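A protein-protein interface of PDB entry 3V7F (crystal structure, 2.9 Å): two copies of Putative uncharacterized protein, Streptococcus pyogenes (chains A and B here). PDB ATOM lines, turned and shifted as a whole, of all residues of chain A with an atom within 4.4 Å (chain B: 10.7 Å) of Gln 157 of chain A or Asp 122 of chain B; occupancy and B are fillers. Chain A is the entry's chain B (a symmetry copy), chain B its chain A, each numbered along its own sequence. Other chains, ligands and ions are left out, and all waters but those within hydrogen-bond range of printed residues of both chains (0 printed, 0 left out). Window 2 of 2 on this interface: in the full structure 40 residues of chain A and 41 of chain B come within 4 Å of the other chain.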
ATOM      1  N   VAL A 141      -9.259  -8.121   5.580  1.00  0.00           N
ATOM      2  CA  VAL A 141      -8.135  -8.161   4.631  1.00  0.00           C
ATOM      3  C   VAL A 141      -7.163  -9.312   4.870  1.00  0.00           C
ATOM      4  O   VAL A 141      -6.786  -9.640   5.998  1.00  0.00           O
ATOM      5  CB  VAL A 141      -7.338  -6.870   4.621  1.00  0.00           C
ATOM      6  CG1 VAL A 141      -6.429  -6.879   3.442  1.00  0.00           C
ATOM      7  CG2 VAL A 141      -8.252  -5.680   4.538  1.00  0.00           C
ATOM      8  N   GLU A 142      -6.776  -9.928   3.773  1.00  0.00           N
ATOM      9  CA  GLU A 142      -5.879 -11.049   3.795  1.00  0.00           C
ATOM     10  C   GLU A 142      -4.466 -10.634   4.226  1.00  0.00           C
ATOM     11  O   GLU A 142      -3.922  -9.627   3.774  1.00  0.00           O
ATOM     12  CB  GLU A 142      -5.851 -11.637   2.396  1.00  0.00           C
ATOM     13  CG  GLU A 142      -5.717 -13.120   2.337  1.00  0.00           C
ATOM     14  CD  GLU A 142      -5.760 -13.633   0.911  1.00  0.00           C
ATOM     15  OE1 GLU A 142      -5.606 -12.816  -0.039  1.00  0.00           O
ATOM     16  OE2 GLU A 142      -5.945 -14.868   0.748  1.00  0.00           O
ATOM     17  N   LEU A 153       3.771  -3.675  -0.314  1.00  0.00           N
ATOM     18  CA  LEU A 153       2.773  -3.822  -1.378  1.00  0.00           C
ATOM     19  C   LEU A 153       1.386  -3.846  -0.803  1.00  0.00           C
ATOM     20  O   LEU A 153       0.465  -3.292  -1.365  1.00  0.00           O
ATOM     21  CB  LEU A 153       2.998  -5.083  -2.196  1.00  0.00           C
ATOM     22  CG  LEU A 153       4.097  -5.055  -3.247  1.00  0.00           C
ATOM     23  CD1 LEU A 153       4.321  -6.460  -3.706  1.00  0.00           C
ATOM     24  CD2 LEU A 153       3.706  -4.190  -4.417  1.00  0.00           C
ATOM     25  N   GLU A 154       1.232  -4.476   0.338  1.00  0.00           N
ATOM     26  CA  GLU A 154      -0.069  -4.493   0.929  1.00  0.00           C
ATOM     27  C   GLU A 154      -0.367  -3.113   1.374  1.00  0.00           C
ATOM     28  O   GLU A 154      -1.441  -2.632   1.078  1.00  0.00           O
ATOM     29  CB  GLU A 154      -0.112  -5.449   2.075  1.00  0.00           C
ATOM     30  CG  GLU A 154       0.468  -6.737   1.684  1.00  0.00           C
ATOM     31  CD  GLU A 154      -0.217  -7.813   2.379  1.00  0.00           C
ATOM     32  OE1 GLU A 154      -0.624  -8.809   1.720  1.00  0.00           O
ATOM     33  OE2 GLU A 154      -0.357  -7.625   3.611  1.00  0.00           O
ATOM     34  N   ILE A 155       0.581  -2.444   2.039  1.00  0.00           N
ATOM     35  CA  ILE A 155       0.322  -1.057   2.458  1.00  0.00           C
ATOM     36  C   ILE A 155       0.000  -0.249   1.219  1.00  0.00           C
ATOM     37  O   ILE A 155      -0.868   0.609   1.234  1.00  0.00           O
ATOM     38  CB  ILE A 155       1.469  -0.423   3.246  1.00  0.00           C
ATOM     39  CG1 ILE A 155       1.823  -1.295   4.452  1.00  0.00           C
ATOM     40  CG2 ILE A 155       1.111   0.950   3.712  1.00  0.00           C
ATOM     41  CD1 ILE A 155       3.180  -0.989   5.082  1.00  0.00           C
ATOM     42  N   LEU A 156       0.670  -0.554   0.114  1.00  0.00           N
ATOM     43  CA  LEU A 156       0.358   0.148  -1.116  1.00  0.00           C
ATOM     44  C   LEU A 156      -1.058  -0.146  -1.569  1.00  0.00           C
ATOM     45  O   LEU A 156      -1.760   0.756  -1.998  1.00  0.00           O
ATOM     46  CB  LEU A 156       1.399  -0.134  -2.195  1.00  0.00           C
ATOM     47  CG  LEU A 156       2.583   0.847  -2.050  1.00  0.00           C
ATOM     48  CD1 LEU A 156       3.861   0.289  -2.650  1.00  0.00           C
ATOM     49  CD2 LEU A 156       2.248   2.155  -2.700  1.00  0.00           C
ATOM     50  N   GLN A 157      -1.491  -1.390  -1.426  1.00  0.00           N
ATOM     51  CA  GLN A 157      -2.803  -1.767  -1.921  1.00  0.00           C
ATOM     52  C   GLN A 157      -3.848  -0.970  -1.142  1.00  0.00           C
ATOM     53  O   GLN A 157      -4.765  -0.351  -1.723  1.00  0.00           O
ATOM     54  CB  GLN A 157      -3.052  -3.271  -1.756  1.00  0.00           C
ATOM     55  CG  GLN A 157      -2.349  -4.211  -2.750  1.00  0.00           C
ATOM     56  CD  GLN A 157      -2.684  -5.711  -2.482  1.00  0.00           C
ATOM     57  OE1 GLN A 157      -3.869  -6.105  -2.261  1.00  0.00           O
ATOM     58  NE2 GLN A 157      -1.638  -6.549  -2.498  1.00  0.00           N
ATOM     59  N   ILE A 158      -3.673  -0.968   0.183  1.00  0.00           N
ATOM     60  CA  ILE A 158      -4.580  -0.278   1.076  1.00  0.00           C
ATOM     61  C   ILE A 158      -4.586   1.197   0.829  1.00  0.00           C
ATOM     62  O   ILE A 158      -5.658   1.785   0.706  1.00  0.00           O
ATOM     63  CB  ILE A 158      -4.287  -0.570   2.484  1.00  0.00           C
ATOM     64  CG1 ILE A 158      -4.964  -1.896   2.796  1.00  0.00           C
ATOM     65  CG2 ILE A 158      -4.966   0.420   3.334  1.00  0.00           C
ATOM     66  CD1 ILE A 158      -4.245  -2.812   3.784  1.00  0.00           C
ATOM     67  N   PHE A 159      -3.406   1.791   0.700  1.00  0.00           N
ATOM     68  CA  PHE A 159      -3.341   3.216   0.383  1.00  0.00           C
ATOM     69  C   PHE A 159      -4.207   3.564  -0.849  1.00  0.00           C
ATOM     70  O   PHE A 159      -4.871   4.635  -0.915  1.00  0.00           O
ATOM     71  CB  PHE A 159      -1.897   3.705   0.202  1.00  0.00           C
ATOM     72  CG  PHE A 159      -1.819   5.103  -0.328  1.00  0.00           C
ATOM     73  CD1 PHE A 159      -2.383   6.164   0.384  1.00  0.00           C
ATOM     74  CD2 PHE A 159      -1.241   5.358  -1.553  1.00  0.00           C
ATOM     75  CE1 PHE A 159      -2.342   7.483  -0.118  1.00  0.00           C
ATOM     76  CE2 PHE A 159      -1.197   6.656  -2.066  1.00  0.00           C
ATOM     77  CZ  PHE A 159      -1.752   7.723  -1.342  1.00  0.00           C
ATOM     78  N   LYS A 160      -4.189   2.623  -1.801  1.00  0.00           N
ATOM     79  CA  LYS A 160      -4.897   2.772  -3.056  1.00  0.00           C
ATOM     80  C   LYS A 160      -6.355   2.709  -2.725  1.00  0.00           C
ATOM     81  O   LYS A 160      -7.147   3.573  -3.127  1.00  0.00           O
ATOM     82  CB  LYS A 160      -4.561   1.632  -4.006  1.00  0.00           C
ATOM     83  CG  LYS A 160      -5.047   1.897  -5.385  1.00  0.00           C
ATOM     84  CD  LYS A 160      -5.294   0.655  -6.202  1.00  0.00           C
ATOM     85  CE  LYS A 160      -6.360   0.993  -7.298  1.00  0.00           C
ATOM     86  NZ  LYS A 160      -6.294   2.419  -7.871  1.00  0.00           N
ATOM     87  N   TYR A 161      -6.689   1.705  -1.921  1.00  0.00           N
ATOM     88  CA  TYR A 161      -8.055   1.469  -1.554  1.00  0.00           C
ATOM     89  C   TYR A 161      -8.733   2.646  -0.848  1.00  0.00           C
ATOM     90  O   TYR A 161      -9.911   2.877  -1.056  1.00  0.00           O
ATOM     91  CB  TYR A 161      -8.175   0.185  -0.746  1.00  0.00           C
ATOM     92  CG  TYR A 161      -9.588  -0.008  -0.341  1.00  0.00           C
ATOM     93  CD1 TYR A 161     -10.547  -0.330  -1.274  1.00  0.00           C
ATOM     94  CD2 TYR A 161      -9.993   0.239   0.975  1.00  0.00           C
ATOM     95  CE1 TYR A 161     -11.865  -0.456  -0.891  1.00  0.00           C
ATOM     96  CE2 TYR A 161     -11.297   0.110   1.359  1.00  0.00           C
ATOM     97  CZ  TYR A 161     -12.217  -0.239   0.431  1.00  0.00           C
ATOM     98  OH  TYR A 161     -13.508  -0.364   0.818  1.00  0.00           O
ATOM     99  N   TYR A 188       4.274  -0.835  -9.538  1.00  0.00           N
ATOM    100  CA  TYR A 188       2.908  -0.744  -8.988  1.00  0.00           C
ATOM    101  C   TYR A 188       2.397   0.711  -8.873  1.00  0.00           C
ATOM    102  O   TYR A 188       1.298   1.036  -9.303  1.00  0.00           O
ATOM    103  CB  TYR A 188       2.845  -1.447  -7.643  1.00  0.00           C
ATOM    104  CG  TYR A 188       1.450  -1.561  -7.044  1.00  0.00           C
ATOM    105  CD1 TYR A 188       0.649  -2.697  -7.259  1.00  0.00           C
ATOM    106  CD2 TYR A 188       0.931  -0.546  -6.246  1.00  0.00           C
ATOM    107  CE1 TYR A 188      -0.647  -2.799  -6.691  1.00  0.00           C
ATOM    108  CE2 TYR A 188      -0.349  -0.631  -5.684  1.00  0.00           C
ATOM    109  CZ  TYR A 188      -1.139  -1.757  -5.899  1.00  0.00           C
ATOM    110  OH  TYR A 188      -2.406  -1.813  -5.322  1.00  0.00           O
ATOM    111  N   VAL B 113     -19.329 -13.225  -0.556  1.00  0.00           N
ATOM    112  CA  VAL B 113     -18.034 -13.542  -1.111  1.00  0.00           C
ATOM    113  C   VAL B 113     -17.932 -13.022  -2.530  1.00  0.00           C
ATOM    114  O   VAL B 113     -16.889 -12.519  -2.935  1.00  0.00           O
ATOM    115  CB  VAL B 113     -17.756 -15.022  -1.104  1.00  0.00           C
ATOM    116  CG1 VAL B 113     -16.372 -15.279  -1.654  1.00  0.00           C
ATOM    117  CG2 VAL B 113     -17.876 -15.551   0.311  1.00  0.00           C
ATOM    118  N   PHE B 114     -18.996 -13.121  -3.314  1.00  0.00           N
ATOM    119  CA  PHE B 114     -18.848 -12.599  -4.663  1.00  0.00           C
ATOM    120  C   PHE B 114     -18.513 -11.117  -4.633  1.00  0.00           C
ATOM    121  O   PHE B 114     -17.588 -10.683  -5.314  1.00  0.00           O
ATOM    122  CB  PHE B 114     -20.022 -12.896  -5.580  1.00  0.00           C
ATOM    123  CG  PHE B 114     -19.753 -12.496  -7.001  1.00  0.00           C
ATOM    124  CD1 PHE B 114     -18.829 -13.217  -7.774  1.00  0.00           C
ATOM    125  CD2 PHE B 114     -20.372 -11.356  -7.560  1.00  0.00           C
ATOM    126  CE1 PHE B 114     -18.533 -12.822  -9.101  1.00  0.00           C
ATOM    127  CE2 PHE B 114     -20.094 -10.952  -8.885  1.00  0.00           C
ATOM    128  CZ  PHE B 114     -19.173 -11.696  -9.663  1.00  0.00           C
ATOM    129  N   GLU B 115     -19.228 -10.358  -3.801  1.00  0.00           N
ATOM    130  CA  GLU B 115     -18.862  -8.958  -3.560  1.00  0.00           C
ATOM    131  C   GLU B 115     -17.450  -8.809  -3.029  1.00  0.00           C
ATOM    132  O   GLU B 115     -16.832  -7.780  -3.233  1.00  0.00           O
ATOM    133  CB  GLU B 115     -19.792  -8.291  -2.565  1.00  0.00           C
ATOM    134  CG  GLU B 115     -21.171  -8.000  -3.049  1.00  0.00           C
ATOM    135  CD  GLU B 115     -21.225  -7.637  -4.505  1.00  0.00           C
ATOM    136  OE1 GLU B 115     -20.669  -6.577  -4.898  1.00  0.00           O
ATOM    137  OE2 GLU B 115     -21.860  -8.434  -5.245  1.00  0.00           O
ATOM    138  N   CYS B 116     -16.951  -9.824  -2.340  1.00  0.00           N
ATOM    139  CA  CYS B 116     -15.620  -9.754  -1.787  1.00  0.00           C
ATOM    140  C   CYS B 116     -14.566  -9.849  -2.838  1.00  0.00           C
ATOM    141  O   CYS B 116     -13.605  -9.098  -2.782  1.00  0.00           O
ATOM    142  CB  CYS B 116     -15.397 -10.838  -0.761  1.00  0.00           C
ATOM    143  SG  CYS B 116     -15.983 -10.346   0.848  1.00  0.00           S
ATOM    144  N   LEU B 117     -14.741 -10.776  -3.784  1.00  0.00           N
ATOM    145  CA  LEU B 117     -13.902 -10.887  -4.992  1.00  0.00           C
ATOM    146  C   LEU B 117     -13.988  -9.651  -5.862  1.00  0.00           C
ATOM    147  O   LEU B 117     -12.982  -9.073  -6.265  1.00  0.00           O
ATOM    148  CB  LEU B 117     -14.387 -12.033  -5.832  1.00  0.00           C
ATOM    149  CG  LEU B 117     -14.162 -13.443  -5.328  1.00  0.00           C
ATOM    150  CD1 LEU B 117     -15.159 -14.382  -6.032  1.00  0.00           C
ATOM    151  CD2 LEU B 117     -12.707 -13.860  -5.568  1.00  0.00           C
ATOM    152  N   GLU B 118     -15.201  -9.235  -6.149  1.00  0.00           N
ATOM    153  CA  GLU B 118     -15.380  -8.016  -6.910  1.00  0.00           C
ATOM    154  C   GLU B 118     -14.768  -6.753  -6.241  1.00  0.00           C
ATOM    155  O   GLU B 118     -14.592  -5.716  -6.901  1.00  0.00           O
ATOM    156  CB  GLU B 118     -16.863  -7.820  -7.248  1.00  0.00           C
ATOM    157  CG  GLU B 118     -17.290  -8.486  -8.554  1.00  0.00           C
ATOM    158  CD  GLU B 118     -17.939  -7.481  -9.471  1.00  0.00           C
ATOM    159  OE1 GLU B 118     -19.127  -7.697  -9.792  1.00  0.00           O
ATOM    160  OE2 GLU B 118     -17.280  -6.454  -9.836  1.00  0.00           O
ATOM    161  N   ASN B 119     -14.461  -6.832  -4.942  1.00  0.00           N
ATOM    162  CA  ASN B 119     -13.806  -5.736  -4.278  1.00  0.00           C
ATOM    163  C   ASN B 119     -12.311  -5.797  -4.572  1.00  0.00           C
ATOM    164  O   ASN B 119     -11.723  -6.904  -4.656  1.00  0.00           O
ATOM    165  CB  ASN B 119     -14.094  -5.750  -2.785  1.00  0.00           C
ATOM    166  CG  ASN B 119     -13.616  -4.482  -2.090  1.00  0.00           C
ATOM    167  OD1 ASN B 119     -12.471  -4.403  -1.688  1.00  0.00           O
ATOM    168  ND2 ASN B 119     -14.487  -3.487  -1.957  1.00  0.00           N
ATOM    169  N   GLU B 120     -11.699  -4.611  -4.728  1.00  0.00           N
ATOM    170  CA  GLU B 120     -10.274  -4.526  -5.099  1.00  0.00           C
ATOM    171  C   GLU B 120      -9.311  -5.165  -4.121  1.00  0.00           C
ATOM    172  O   GLU B 120      -8.238  -5.609  -4.499  1.00  0.00           O
ATOM    173  CB  GLU B 120      -9.827  -3.101  -5.464  1.00  0.00           C
ATOM    174  CG  GLU B 120      -9.592  -2.130  -4.336  1.00  0.00           C
ATOM    175  CD  GLU B 120      -9.399  -0.695  -4.854  1.00  0.00           C
ATOM    176  OE1 GLU B 120      -8.227  -0.226  -4.941  1.00  0.00           O
ATOM    177  OE2 GLU B 120     -10.429  -0.049  -5.187  1.00  0.00           O
ATOM    178  N   LEU B 121      -9.712  -5.221  -2.870  1.00  0.00           N
ATOM    179  CA  LEU B 121      -8.868  -5.752  -1.843  1.00  0.00           C
ATOM    180  C   LEU B 121      -8.984  -7.269  -1.811  1.00  0.00           C
ATOM    181  O   LEU B 121     -10.062  -7.790  -2.107  1.00  0.00           O
ATOM    182  CB  LEU B 121      -9.311  -5.165  -0.510  1.00  0.00           C
ATOM    183  CG  LEU B 121      -8.978  -3.699  -0.301  1.00  0.00           C
ATOM    184  CD1 LEU B 121      -9.652  -3.255   0.953  1.00  0.00           C
ATOM    185  CD2 LEU B 121      -7.504  -3.596  -0.165  1.00  0.00           C
ATOM    186  N   ASP B 122      -7.895  -7.970  -1.459  1.00  0.00           N
ATOM    187  CA  ASP B 122      -7.936  -9.423  -1.230  1.00  0.00           C
ATOM    188  C   ASP B 122      -8.525  -9.687   0.128  1.00  0.00           C
ATOM    189  O   ASP B 122      -7.850  -9.486   1.128  1.00  0.00           O
ATOM    190  CB  ASP B 122      -6.539 -10.039  -1.309  1.00  0.00           C
ATOM    191  CG  ASP B 122      -5.938  -9.944  -2.703  1.00  0.00           C
ATOM    192  OD1 ASP B 122      -6.661 -10.265  -3.682  1.00  0.00           O
ATOM    193  OD2 ASP B 122      -4.748  -9.537  -2.829  1.00  0.00           O
ATOM    194  N   LEU B 123      -9.785 -10.115   0.179  1.00  0.00           N
ATOM    195  CA  LEU B 123     -10.479 -10.263   1.453  1.00  0.00           C
ATOM    196  C   LEU B 123     -10.651 -11.711   1.826  1.00  0.00           C
ATOM    197  O   LEU B 123     -10.878 -12.555   0.960  1.00  0.00           O
ATOM    198  CB  LEU B 123     -11.849  -9.631   1.375  1.00  0.00           C
ATOM    199  CG  LEU B 123     -11.931  -8.222   0.841  1.00  0.00           C
ATOM    200  CD1 LEU B 123     -13.292  -7.953   0.352  1.00  0.00           C
ATOM    201  CD2 LEU B 123     -11.555  -7.224   1.916  1.00  0.00           C
ATOM    202  N   GLU B 124     -10.564 -12.027   3.112  1.00  0.00           N
ATOM    203  CA  GLU B 124     -10.948 -13.360   3.541  1.00  0.00           C
ATOM    204  C   GLU B 124     -12.134 -13.244   4.439  1.00  0.00           C
ATOM    205  O   GLU B 124     -12.572 -12.150   4.731  1.00  0.00           O
ATOM    206  CB  GLU B 124      -9.811 -14.117   4.218  1.00  0.00           C
ATOM    207  CG  GLU B 124      -9.213 -13.446   5.431  1.00  0.00           C
ATOM    208  CD  GLU B 124      -8.019 -14.232   6.012  1.00  0.00           C
ATOM    209  OE1 GLU B 124      -7.507 -15.154   5.324  1.00  0.00           O
ATOM    210  OE2 GLU B 124      -7.593 -13.914   7.153  1.00  0.00           O
ATOM    211  N   TYR B 125     -12.651 -14.376   4.882  1.00  0.00           N
ATOM    212  CA  TYR B 125     -13.867 -14.407   5.606  1.00  0.00           C
ATOM    213  C   TYR B 125     -13.952 -15.729   6.334  1.00  0.00           C
ATOM    214  O   TYR B 125     -13.128 -16.617   6.142  1.00  0.00           O
ATOM    215  CB  TYR B 125     -15.016 -14.232   4.634  1.00  0.00           C
ATOM    216  CG  TYR B 125     -14.915 -15.120   3.427  1.00  0.00           C
ATOM    217  CD1 TYR B 125     -14.430 -14.638   2.227  1.00  0.00           C
ATOM    218  CD2 TYR B 125     -15.315 -16.454   3.489  1.00  0.00           C
ATOM    219  CE1 TYR B 125     -14.344 -15.472   1.109  1.00  0.00           C
ATOM    220  CE2 TYR B 125     -15.250 -17.282   2.392  1.00  0.00           C
ATOM    221  CZ  TYR B 125     -14.762 -16.790   1.207  1.00  0.00           C
ATOM    222  OH  TYR B 125     -14.682 -17.630   0.123  1.00  0.00           O
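O of Asp 122 of chain B is in hydrogen-bond range of N of Glu 142 of chain A (2.9 Å).
The side-chain amide oxygen (OD1) of Asn 119 of chain B is in hydrogen-bond range of the backbone NH (N) of Leu 121 of chain B (3.1 Å).
Val 141 of chain A touches Asp 122 of chain B (CA to O, 3.8 Å). Asp 122 of chain B touches Gln 157 of chain A. OE1 of Glu 120 of chain B touches CE of Lys 160 of chain A, at 3.2 Å. CG of Glu 120 of chain B touches CD1 of Tyr 161 of chain A, at 3.7 Å. CG of Tyr 161 of chain A touches CD1 of Leu 121 of chain B, 3.5 Å away.
Of chain B, only Asp 122 (3.8 Å) comes within 4 Å of Val 141 of chain A. Of chain B, only Asp 122 comes within 4 Å of Glu 142 of chain A. Leu 153 of chain A touches none of the printed residues of chain B. No residue of chain B comes within 4 Å of Glu 154 of chain A. Gln 157 of chain A touches just one residue of chain B: Asp 122 (3.6 Å). Ile 158 of chain A touches none of the printed residues of chain B. Printed residues of chain B within 4 Å of Lys 160 of chain A: Glu 120. Printed residues of chain B within 4 Å of Tyr 161 of chain A: Glu 120 (3.7 Å) and Leu 121 (3.5 Å). Tyr 188 of chain A touches none of the printed residues of chain B. Printed residues of chain A within 4 Å of Glu 120 of chain B: Lys 160 and Tyr 161. Of the printed residues of chain A, Leu 121 of chain B touches Tyr 161 (3.5 Å). Asp 122 of chain B touches just these residues of chain A: Val 141 (3.8 Å), Glu 142 (2.9 Å) and Gln 157 (3.6 Å). Tyr 125 of chain B touches none of the printed residues of chain A. The nearest residue of chain B that does not touch Gln 157 of chain A is Leu 121 of chain B (4.5 Å).
Among the printed residues, no Asp or Glu carboxylate lies within 4 Å of a Lys or Arg side-chain nitrogen of the other chain.
No position is printed for both chains. Of the 6 pairs that touch across the chains among the printed residues, none has its exchanged pair printed and touching as well.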
